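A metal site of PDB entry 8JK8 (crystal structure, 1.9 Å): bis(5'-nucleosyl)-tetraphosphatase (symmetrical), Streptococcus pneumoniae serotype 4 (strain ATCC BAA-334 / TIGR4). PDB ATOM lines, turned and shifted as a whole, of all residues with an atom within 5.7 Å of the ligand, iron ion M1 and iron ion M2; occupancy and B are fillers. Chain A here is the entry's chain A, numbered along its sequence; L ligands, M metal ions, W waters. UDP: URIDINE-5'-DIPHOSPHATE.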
ATOM      1  N   ARG A  26     -36.173 -10.211 -34.166  1.00  0.00           N
ATOM      2  CA  ARG A  26     -34.954  -9.996 -33.397  1.00  0.00           C
ATOM      3  C   ARG A  26     -34.915  -8.588 -32.782  1.00  0.00           C
ATOM      4  O   ARG A  26     -34.468  -8.438 -31.639  1.00  0.00           O
ATOM      5  CB  ARG A  26     -33.716 -10.309 -34.242  1.00  0.00           C
ATOM      6  CG  ARG A  26     -32.375 -10.217 -33.527  1.00  0.00           C
ATOM      7  CD  ARG A  26     -32.293 -11.149 -32.325  1.00  0.00           C
ATOM      8  NE  ARG A  26     -32.421 -12.527 -32.764  1.00  0.00           N
ATOM      9  CZ  ARG A  26     -32.514 -13.590 -31.977  1.00  0.00           C
ATOM     10  NH1 ARG A  26     -32.610 -14.788 -32.513  1.00  0.00           N
ATOM     11  NH2 ARG A  26     -32.503 -13.450 -30.652  1.00  0.00           N
ATOM     12  N   HIS A  29     -37.316  -8.523 -29.939  1.00  0.00           N
ATOM     13  CA  HIS A  29     -36.613  -9.229 -28.855  1.00  0.00           C
ATOM     14  C   HIS A  29     -35.708  -8.253 -28.080  1.00  0.00           C
ATOM     15  O   HIS A  29     -35.779  -8.188 -26.857  1.00  0.00           O
ATOM     16  CB  HIS A  29     -35.816 -10.438 -29.379  1.00  0.00           C
ATOM     17  CG  HIS A  29     -34.796 -10.989 -28.411  1.00  0.00           C
ATOM     18  ND1 HIS A  29     -35.155 -11.564 -27.200  1.00  0.00           N
ATOM     19  CD2 HIS A  29     -33.444 -11.054 -28.457  1.00  0.00           C
ATOM     20  CE1 HIS A  29     -34.075 -11.961 -26.563  1.00  0.00           C
ATOM     21  NE2 HIS A  29     -33.025 -11.660 -27.304  1.00  0.00           N
ATOM     22  N   VAL A  33     -35.860  -7.107 -24.227  1.00  0.00           N
ATOM     23  CA  VAL A  33     -34.731  -7.224 -23.302  1.00  0.00           C
ATOM     24  C   VAL A  33     -34.363  -5.885 -22.663  1.00  0.00           C
ATOM     25  O   VAL A  33     -34.042  -5.838 -21.491  1.00  0.00           O
ATOM     26  CB  VAL A  33     -33.496  -7.880 -23.971  1.00  0.00           C
ATOM     27  CG1 VAL A  33     -32.322  -7.950 -23.001  1.00  0.00           C
ATOM     28  CG2 VAL A  33     -33.831  -9.302 -24.408  1.00  0.00           C
ATOM     29  N   HIS A  58     -27.692  -6.113 -26.823  1.00  0.00           N
ATOM     30  CA  HIS A  58     -27.025  -7.404 -26.590  1.00  0.00           C
ATOM     31  C   HIS A  58     -26.947  -8.279 -27.869  1.00  0.00           C
ATOM     32  O   HIS A  58     -25.939  -8.969 -28.090  1.00  0.00           O
ATOM     33  CB  HIS A  58     -27.673  -8.151 -25.415  1.00  0.00           C
ATOM     34  CG  HIS A  58     -28.920  -8.875 -25.793  1.00  0.00           C
ATOM     35  ND1 HIS A  58     -30.096  -8.222 -26.072  1.00  0.00           N
ATOM     36  CD2 HIS A  58     -29.151 -10.195 -25.981  1.00  0.00           C
ATOM     37  CE1 HIS A  58     -31.013  -9.113 -26.422  1.00  0.00           C
ATOM     38  NE2 HIS A  58     -30.468 -10.308 -26.390  1.00  0.00           N
ATOM     39  N   ASP A  59     -27.987  -8.227 -28.710  1.00  0.00           N
ATOM     40  CA  ASP A  59     -28.094  -9.042 -29.926  1.00  0.00           C
ATOM     41  C   ASP A  59     -27.883  -8.236 -31.201  1.00  0.00           C
ATOM     42  O   ASP A  59     -28.257  -8.673 -32.292  1.00  0.00           O
ATOM     43  CB  ASP A  59     -29.426  -9.811 -29.991  1.00  0.00           C
ATOM     44  CG  ASP A  59     -29.374 -11.158 -29.279  1.00  0.00           C
ATOM     45  OD1 ASP A  59     -28.290 -11.625 -28.905  1.00  0.00           O
ATOM     46  OD2 ASP A  59     -30.443 -11.718 -29.029  1.00  0.00           O
ATOM     47  N   LYS A  62     -26.232 -10.140 -34.012  1.00  0.00           N
ATOM     48  CA  LYS A  62     -26.814 -11.483 -34.218  1.00  0.00           C
ATOM     49  C   LYS A  62     -26.777 -11.946 -35.685  1.00  0.00           C
ATOM     50  O   LYS A  62     -26.653 -13.143 -35.943  1.00  0.00           O
ATOM     51  CB  LYS A  62     -28.244 -11.564 -33.655  1.00  0.00           C
ATOM     52  CG  LYS A  62     -28.896 -12.947 -33.633  1.00  0.00           C
ATOM     53  CD  LYS A  62     -28.255 -13.913 -32.632  1.00  0.00           C
ATOM     54  CE  LYS A  62     -28.876 -15.295 -32.739  1.00  0.00           C
ATOM     55  NZ  LYS A  62     -28.737 -16.122 -31.503  1.00  0.00           N
ATOM     56  N   TRP A  85     -15.776 -22.368 -33.072  1.00  0.00           N
ATOM     57  CA  TRP A  85     -17.149 -22.180 -32.633  1.00  0.00           C
ATOM     58  C   TRP A  85     -17.921 -21.486 -33.742  1.00  0.00           C
ATOM     59  O   TRP A  85     -17.506 -21.547 -34.899  1.00  0.00           O
ATOM     60  CB  TRP A  85     -17.135 -21.432 -31.302  1.00  0.00           C
ATOM     61  CG  TRP A  85     -16.388 -22.274 -30.312  1.00  0.00           C
ATOM     62  CD1 TRP A  85     -15.055 -22.211 -30.026  1.00  0.00           C
ATOM     63  CD2 TRP A  85     -16.915 -23.338 -29.535  1.00  0.00           C
ATOM     64  NE1 TRP A  85     -14.729 -23.170 -29.103  1.00  0.00           N
ATOM     65  CE2 TRP A  85     -15.850 -23.876 -28.772  1.00  0.00           C
ATOM     66  CE3 TRP A  85     -18.201 -23.891 -29.382  1.00  0.00           C
ATOM     67  CZ2 TRP A  85     -16.022 -24.925 -27.869  1.00  0.00           C
ATOM     68  CZ3 TRP A  85     -18.366 -24.929 -28.484  1.00  0.00           C
ATOM     69  CH2 TRP A  85     -17.283 -25.448 -27.753  1.00  0.00           C
ATOM     70  N   ASN A  88     -23.552 -18.427 -32.191  1.00  0.00           N
ATOM     71  CA  ASN A  88     -23.982 -18.535 -30.791  1.00  0.00           C
ATOM     72  C   ASN A  88     -22.990 -17.962 -29.784  1.00  0.00           C
ATOM     73  O   ASN A  88     -23.381 -17.145 -28.960  1.00  0.00           O
ATOM     74  CB  ASN A  88     -24.323 -19.975 -30.449  1.00  0.00           C
ATOM     75  CG  ASN A  88     -25.597 -20.452 -31.137  1.00  0.00           C
ATOM     76  OD1 ASN A  88     -26.381 -19.649 -31.653  1.00  0.00           O
ATOM     77  ND2 ASN A  88     -25.817 -21.765 -31.114  1.00  0.00           N
ATOM     78  N   VAL A  89     -21.731 -18.392 -29.888  1.00  0.00           N
ATOM     79  CA  VAL A  89     -20.633 -17.862 -29.080  1.00  0.00           C
ATOM     80  C   VAL A  89     -20.210 -16.473 -29.573  1.00  0.00           C
ATOM     81  O   VAL A  89     -19.914 -15.582 -28.770  1.00  0.00           O
ATOM     82  CB  VAL A  89     -19.403 -18.827 -29.050  1.00  0.00           C
ATOM     83  CG1 VAL A  89     -18.211 -18.210 -28.332  1.00  0.00           C
ATOM     84  CG2 VAL A  89     -19.765 -20.137 -28.355  1.00  0.00           C
ATOM     85  N   HIS A  91     -21.643 -13.857 -31.408  1.00  0.00           N
ATOM     86  CA  HIS A  91     -22.457 -12.633 -31.506  1.00  0.00           C
ATOM     87  C   HIS A  91     -22.291 -11.718 -30.264  1.00  0.00           C
ATOM     88  O   HIS A  91     -22.218 -10.506 -30.400  1.00  0.00           O
ATOM     89  CB  HIS A  91     -23.918 -12.939 -31.930  1.00  0.00           C
ATOM     90  CG  HIS A  91     -24.799 -13.452 -30.835  1.00  0.00           C
ATOM     91  ND1 HIS A  91     -24.911 -14.803 -30.543  1.00  0.00           N
ATOM     92  CD2 HIS A  91     -25.648 -12.817 -29.995  1.00  0.00           C
ATOM     93  CE1 HIS A  91     -25.769 -14.958 -29.542  1.00  0.00           C
ATOM     94  NE2 HIS A  91     -26.216 -13.770 -29.192  1.00  0.00           N
ATOM     95  N   HIS A 117     -23.279 -12.364 -22.493  1.00  0.00           N
ATOM     96  CA  HIS A 117     -24.747 -12.567 -22.368  1.00  0.00           C
ATOM     97  C   HIS A 117     -25.226 -13.998 -22.696  1.00  0.00           C
ATOM     98  O   HIS A 117     -26.268 -14.423 -22.191  1.00  0.00           O
ATOM     99  CB  HIS A 117     -25.566 -11.503 -23.155  1.00  0.00           C
ATOM    100  CG  HIS A 117     -25.774 -11.843 -24.606  1.00  0.00           C
ATOM    101  ND1 HIS A 117     -24.962 -11.340 -25.605  1.00  0.00           N
ATOM    102  CD2 HIS A 117     -26.710 -12.612 -25.229  1.00  0.00           C
ATOM    103  CE1 HIS A 117     -25.372 -11.807 -26.774  1.00  0.00           C
ATOM    104  NE2 HIS A 117     -26.430 -12.574 -26.581  1.00  0.00           N
ATOM    105  N   THR A 118     -24.478 -14.706 -23.543  1.00  0.00           N
ATOM    106  CA  THR A 118     -24.840 -16.068 -24.028  1.00  0.00           C
ATOM    107  C   THR A 118     -24.248 -17.151 -23.113  1.00  0.00           C
ATOM    108  O   THR A 118     -24.953 -18.073 -22.696  1.00  0.00           O
ATOM    109  CB  THR A 118     -24.375 -16.325 -25.499  1.00  0.00           C
ATOM    110  OG1 THR A 118     -24.857 -15.294 -26.370  1.00  0.00           O
ATOM    111  CG2 THR A 118     -24.873 -17.685 -26.015  1.00  0.00           C
ATOM    112  N   VAL A 119     -22.964 -17.010 -22.808  1.00  0.00           N
ATOM    113  CA  VAL A 119     -22.162 -18.033 -22.115  1.00  0.00           C
ATOM    114  C   VAL A 119     -21.935 -17.793 -20.617  1.00  0.00           C
ATOM    115  O   VAL A 119     -21.531 -18.713 -19.893  1.00  0.00           O
ATOM    116  CB  VAL A 119     -20.781 -18.218 -22.791  1.00  0.00           C
ATOM    117  CG1 VAL A 119     -20.962 -18.703 -24.223  1.00  0.00           C
ATOM    118  CG2 VAL A 119     -19.943 -16.931 -22.739  1.00  0.00           C
ATOM    119  N   ASP A 135     -32.541 -11.461 -21.074  1.00  0.00           N
ATOM    120  CA  ASP A 135     -32.548 -12.076 -22.404  1.00  0.00           C
ATOM    121  C   ASP A 135     -33.548 -13.262 -22.449  1.00  0.00           C
ATOM    122  O   ASP A 135     -34.324 -13.452 -23.419  1.00  0.00           O
ATOM    123  CB  ASP A 135     -31.115 -12.532 -22.710  1.00  0.00           C
ATOM    124  CG  ASP A 135     -30.957 -13.086 -24.103  1.00  0.00           C
ATOM    125  OD1 ASP A 135     -31.725 -12.669 -25.003  1.00  0.00           O
ATOM    126  OD2 ASP A 135     -30.083 -13.951 -24.286  1.00  0.00           O
ATOM    127  N   ARG A 141     -40.853 -13.800 -25.081  1.00  0.00           N
ATOM    128  CA  ARG A 141     -40.499 -15.224 -24.993  1.00  0.00           C
ATOM    129  C   ARG A 141     -41.677 -16.027 -24.480  1.00  0.00           C
ATOM    130  O   ARG A 141     -42.418 -15.562 -23.617  1.00  0.00           O
ATOM    131  CB  ARG A 141     -39.314 -15.474 -24.062  1.00  0.00           C
ATOM    132  CG  ARG A 141     -38.062 -14.646 -24.297  1.00  0.00           C
ATOM    133  CD  ARG A 141     -37.213 -15.071 -25.487  1.00  0.00           C
ATOM    134  NE  ARG A 141     -36.836 -16.479 -25.489  1.00  0.00           N
ATOM    135  CZ  ARG A 141     -35.596 -16.904 -25.255  1.00  0.00           C
ATOM    136  NH1 ARG A 141     -35.338 -18.200 -25.319  1.00  0.00           N
ATOM    137  NH2 ARG A 141     -34.620 -16.048 -24.975  1.00  0.00           N
ATOM    138  N   GLU A 164     -31.469 -20.728 -15.657  1.00  0.00           N
ATOM    139  CA  GLU A 164     -31.221 -20.544 -17.091  1.00  0.00           C
ATOM    140  C   GLU A 164     -30.010 -21.361 -17.574  1.00  0.00           C
ATOM    141  O   GLU A 164     -30.105 -22.075 -18.592  1.00  0.00           O
ATOM    142  CB  GLU A 164     -31.039 -19.075 -17.439  1.00  0.00           C
ATOM    143  CG  GLU A 164     -30.661 -18.862 -18.901  1.00  0.00           C
ATOM    144  CD  GLU A 164     -30.442 -17.426 -19.290  1.00  0.00           C
ATOM    145  OE1 GLU A 164     -30.710 -16.501 -18.487  1.00  0.00           O
ATOM    146  OE2 GLU A 164     -30.031 -17.228 -20.459  1.00  0.00           O
ATOM    147  N   THR A 168     -29.960 -24.503 -20.258  1.00  0.00           N
ATOM    148  CA  THR A 168     -29.150 -24.376 -21.467  1.00  0.00           C
ATOM    149  C   THR A 168     -28.226 -25.576 -21.635  1.00  0.00           C
ATOM    150  O   THR A 168     -28.185 -26.179 -22.710  1.00  0.00           O
ATOM    151  CB  THR A 168     -28.357 -23.050 -21.431  1.00  0.00           C
ATOM    152  OG1 THR A 168     -29.299 -21.979 -21.530  1.00  0.00           O
ATOM    153  CG2 THR A 168     -27.343 -22.945 -22.574  1.00  0.00           C
ATOM    154  N   TYR A 171     -30.339 -28.755 -22.401  1.00  0.00           N
ATOM    155  CA  TYR A 171     -30.827 -28.727 -23.787  1.00  0.00           C
ATOM    156  C   TYR A 171     -29.706 -28.960 -24.821  1.00  0.00           C
ATOM    157  O   TYR A 171     -29.925 -29.699 -25.775  1.00  0.00           O
ATOM    158  CB  TYR A 171     -31.579 -27.419 -24.083  1.00  0.00           C
ATOM    159  CG  TYR A 171     -31.921 -27.180 -25.550  1.00  0.00           C
ATOM    160  CD1 TYR A 171     -33.090 -27.715 -26.116  1.00  0.00           C
ATOM    161  CD2 TYR A 171     -31.095 -26.392 -26.362  1.00  0.00           C
ATOM    162  CE1 TYR A 171     -33.418 -27.487 -27.448  1.00  0.00           C
ATOM    163  CE2 TYR A 171     -31.401 -26.163 -27.700  1.00  0.00           C
ATOM    164  CZ  TYR A 171     -32.571 -26.703 -28.239  1.00  0.00           C
ATOM    165  OH  TYR A 171     -32.861 -26.462 -29.568  1.00  0.00           O
ATOM    166  N   LEU A 172     -28.538 -28.332 -24.627  1.00  0.00           N
ATOM    167  CA  LEU A 172     -27.416 -28.570 -25.533  1.00  0.00           C
ATOM    168  C   LEU A 172     -27.003 -30.046 -25.554  1.00  0.00           C
ATOM    169  O   LEU A 172     -26.763 -30.608 -26.631  1.00  0.00           O
ATOM    170  CB  LEU A 172     -26.216 -27.663 -25.217  1.00  0.00           C
ATOM    171  CG  LEU A 172     -26.428 -26.175 -25.477  1.00  0.00           C
ATOM    172  CD1 LEU A 172     -25.297 -25.389 -24.853  1.00  0.00           C
ATOM    173  CD2 LEU A 172     -26.554 -25.847 -26.973  1.00  0.00           C
ATOM    174  N   PRO A 178     -22.106 -29.063 -29.197  1.00  0.00           N
ATOM    175  CA  PRO A 178     -20.946 -28.722 -28.356  1.00  0.00           C
ATOM    176  C   PRO A 178     -21.298 -27.637 -27.326  1.00  0.00           C
ATOM    177  O   PRO A 178     -22.168 -26.802 -27.579  1.00  0.00           O
ATOM    178  CB  PRO A 178     -19.931 -28.161 -29.354  1.00  0.00           C
ATOM    179  CG  PRO A 178     -20.352 -28.648 -30.699  1.00  0.00           C
ATOM    180  CD  PRO A 178     -21.842 -28.835 -30.630  1.00  0.00           C
ATOM    181  N   ILE A 179     -20.662 -27.703 -26.166  1.00  0.00           N
ATOM    182  CA  ILE A 179     -20.919 -26.753 -25.079  1.00  0.00           C
ATOM    183  C   ILE A 179     -19.663 -25.927 -24.840  1.00  0.00           C
ATOM    184  O   ILE A 179     -18.603 -26.476 -24.481  1.00  0.00           O
ATOM    185  CB  ILE A 179     -21.371 -27.482 -23.781  1.00  0.00           C
ATOM    186  CG1 ILE A 179     -22.751 -28.138 -23.986  1.00  0.00           C
ATOM    187  CG2 ILE A 179     -21.371 -26.537 -22.573  1.00  0.00           C
ATOM    188  CD1 ILE A 179     -23.102 -29.244 -22.989  1.00  0.00           C
ATOM    189  N   TYR A 180     -19.767 -24.617 -25.035  1.00  0.00           N
ATOM    190  CA  TYR A 180     -18.636 -23.731 -24.825  1.00  0.00           C
ATOM    191  C   TYR A 180     -18.112 -23.874 -23.402  1.00  0.00           C
ATOM    192  O   TYR A 180     -18.912 -23.810 -22.454  1.00  0.00           O
ATOM    193  CB  TYR A 180     -19.025 -22.276 -25.131  1.00  0.00           C
ATOM    194  CG  TYR A 180     -17.824 -21.384 -25.262  1.00  0.00           C
ATOM    195  CD1 TYR A 180     -16.893 -21.598 -26.269  1.00  0.00           C
ATOM    196  CD2 TYR A 180     -17.628 -20.313 -24.387  1.00  0.00           C
ATOM    197  CE1 TYR A 180     -15.782 -20.784 -26.402  1.00  0.00           C
ATOM    198  CE2 TYR A 180     -16.524 -19.479 -24.523  1.00  0.00           C
ATOM    199  CZ  TYR A 180     -15.603 -19.727 -25.523  1.00  0.00           C
ATOM    200  OH  TYR A 180     -14.499 -18.922 -25.664  1.00  0.00           O
ATOM    201  N   THR A 183     -19.401 -21.712 -20.638  1.00  0.00           N
ATOM    202  CA  THR A 183     -20.767 -22.021 -20.163  1.00  0.00           C
ATOM    203  C   THR A 183     -20.716 -22.958 -18.955  1.00  0.00           C
ATOM    204  O   THR A 183     -21.488 -22.763 -17.998  1.00  0.00           O
ATOM    205  CB  THR A 183     -21.670 -22.537 -21.316  1.00  0.00           C
ATOM    206  OG1 THR A 183     -21.723 -21.522 -22.317  1.00  0.00           O
ATOM    207  CG2 THR A 183     -23.121 -22.875 -20.849  1.00  0.00           C
HETATM  208  N1  UDP L   1     -25.470 -21.776 -26.957  1.00  0.00           N
HETATM  209  C2  UDP L   1     -25.293 -21.450 -25.582  1.00  0.00           C
HETATM  210  N3  UDP L   1     -24.181 -21.856 -24.917  1.00  0.00           N
HETATM  211  C4  UDP L   1     -23.224 -22.583 -25.525  1.00  0.00           C
HETATM  212  C5  UDP L   1     -23.351 -22.933 -26.882  1.00  0.00           C
HETATM  213  C6  UDP L   1     -24.498 -22.511 -27.581  1.00  0.00           C
HETATM  214  O2  UDP L   1     -26.138 -20.778 -24.951  1.00  0.00           O
HETATM  215  O4  UDP L   1     -22.210 -22.947 -24.869  1.00  0.00           O
HETATM  216  C1' UDP L   1     -26.674 -21.353 -27.736  1.00  0.00           C
HETATM  217  C2' UDP L   1     -28.027 -21.418 -27.011  1.00  0.00           C
HETATM  218  O2' UDP L   1     -28.469 -22.757 -26.768  1.00  0.00           O
HETATM  219  C3' UDP L   1     -28.939 -20.555 -27.892  1.00  0.00           C
HETATM  220  C4' UDP L   1     -27.964 -19.636 -28.620  1.00  0.00           C
HETATM  221  O4' UDP L   1     -26.636 -19.994 -28.193  1.00  0.00           O
HETATM  222  O3' UDP L   1     -29.657 -21.315 -28.875  1.00  0.00           O
HETATM  223  C5' UDP L   1     -28.234 -18.154 -28.423  1.00  0.00           C
HETATM  224  O5' UDP L   1     -28.173 -17.802 -27.038  1.00  0.00           O
HETATM  225  PA  UDP L   1     -28.486 -16.313 -26.475  1.00  0.00           P
HETATM  226  O1A UDP L   1     -27.418 -15.402 -27.008  1.00  0.00           O
HETATM  227  O2A UDP L   1     -28.579 -16.442 -24.955  1.00  0.00           O
HETATM  228  O3A UDP L   1     -30.000 -15.998 -27.043  1.00  0.00           O
HETATM  229  PB  UDP L   1     -30.560 -15.297 -28.426  1.00  0.00           P
HETATM  230  O1B UDP L   1     -29.414 -14.520 -29.082  1.00  0.00           O
HETATM  231  O2B UDP L   1     -31.670 -14.385 -27.889  1.00  0.00           O
HETATM  232  O3B UDP L   1     -31.106 -16.436 -29.278  1.00  0.00           O
HETATM  233 FE    FE M   1     -31.141 -12.272 -27.031  1.00  0.00          FE
HETATM  234 FE    FE M   2     -27.800 -13.438 -27.834  1.00  0.00          FE
HETATM  235  O   HOH W   1     -27.441 -18.619 -23.553  1.00  0.00           O
HETATM  236  O   HOH W   2     -31.957 -16.612 -24.058  1.00  0.00           O
HETATM  237  O   HOH W   3     -34.420 -15.000 -28.125  1.00  0.00           O
HETATM  238  O   HOH W   4     -28.618 -15.332 -22.183  1.00  0.00           O
HETATM  239  O   HOH W   5     -29.489 -13.104 -26.759  1.00  0.00           O
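The side-chain hydroxyl (OG1) of Thr 118 sits close to an oxygen (O1A) of the ligand (2.6 Å).
O4 of the ligand is in hydrogen-bond range of N of Tyr 180, at 3.0 Å.
The side-chain hydroxyl (OG1) of Thr 183 sits at hydrogen-bond distance from an oxygen (O4) of the ligand, 3.0 Å away.
NZ of Lys 62 lies within salt-bridge range of O3B of the ligand (3.3 Å).
NH2 of Arg 26 is in salt-bridge range of O3B of the ligand.
The side-chain amide oxygen (OD1) of Asn 88 sits close to an oxygen (O4') of the ligand (3.5 Å).
Water W5 bridges OD2 of Asp 135 (2.7 Å) and O3A of the ligand (3.0 Å).
Water W1 lies within hydrogen-bond range of the backbone carbonyl oxygen (O) of Thr 118 (2.7 Å) and an oxygen (O2A) of the ligand (2.8 Å).
Water W2 lies within hydrogen-bond range of the guanidinium group (NH2) of Arg 141, the side-chain carboxylate (OD2) of Asp 135 and an oxygen (O2A) of the ligand.
Merely in contact with the ligand: Thr 168 (3.4 Å), Leu 172 (3.6 Å) and Ile 179 (3.9 Å).
Hydrophobic or aromatic side chains within 4 Å of the ligand: His 29, His 91, His 117, Leu 172 and Tyr 180.
Iron ion M2 is bound by water W5 (2.0 Å), NE2 of His 117 (2.0 Å), NE2 of His 91 (2.1 Å), OD1 of Asp 59 (2.2 Å), O1A of the ligand (2.2 Å) and O1B of the ligand (2.3 Å).
Iron ion M2 has six donor atoms within binding distance.
Merely in contact with iron ion M2: Thr 118 (3.8 Å).
Of the 23 residues printed, 5 come within 4 Å of iron ion M2.
NE2 of His 91 lies close to OG1 of Thr 118, 3.5 Å away.
The backbone carbonyl oxygen (O) of Asn 88 is in hydrogen-bond range of a ring nitrogen (ND1) of His 91, 3.2 Å away.
O of Asp 135 sits at hydrogen-bond distance from NH2 of Arg 141 (3.0 Å).
The side-chain hydroxyl (OG1) of Thr 118 lies close to a ring nitrogen (NE2) of His 117 (3.1 Å).
The side-chain hydroxyl (OG1) of Thr 168 sits at hydrogen-bond distance from the backbone carbonyl oxygen (O) of Glu 164 (3.0 Å).
NH2 of Arg 26 sits close to OD2 of Asp 59 (3.1 Å).
Four residues have an atom within 4 Å of iron ion M1: His 29, His 58, Asp 59 and Asp 135.
Iron ion M1 is bound by water W5 (1.9 Å).
Iron ion M1 is bound by NE2 of His 29 (2.0 Å).
The side-chain carboxylate (OD1) of Asp 135 is bound to iron ion M1, 2.1 Å away.
A ring nitrogen (NE2) of His 58 binds iron ion M1, at 2.2 Å.
OD2 of Asp 59 is bound to iron ion M1.
Iron ion M1 is bound by an oxygen (O2B) of the ligand, at 2.3 Å.
Iron ion M1 has six donor atoms within binding distance.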
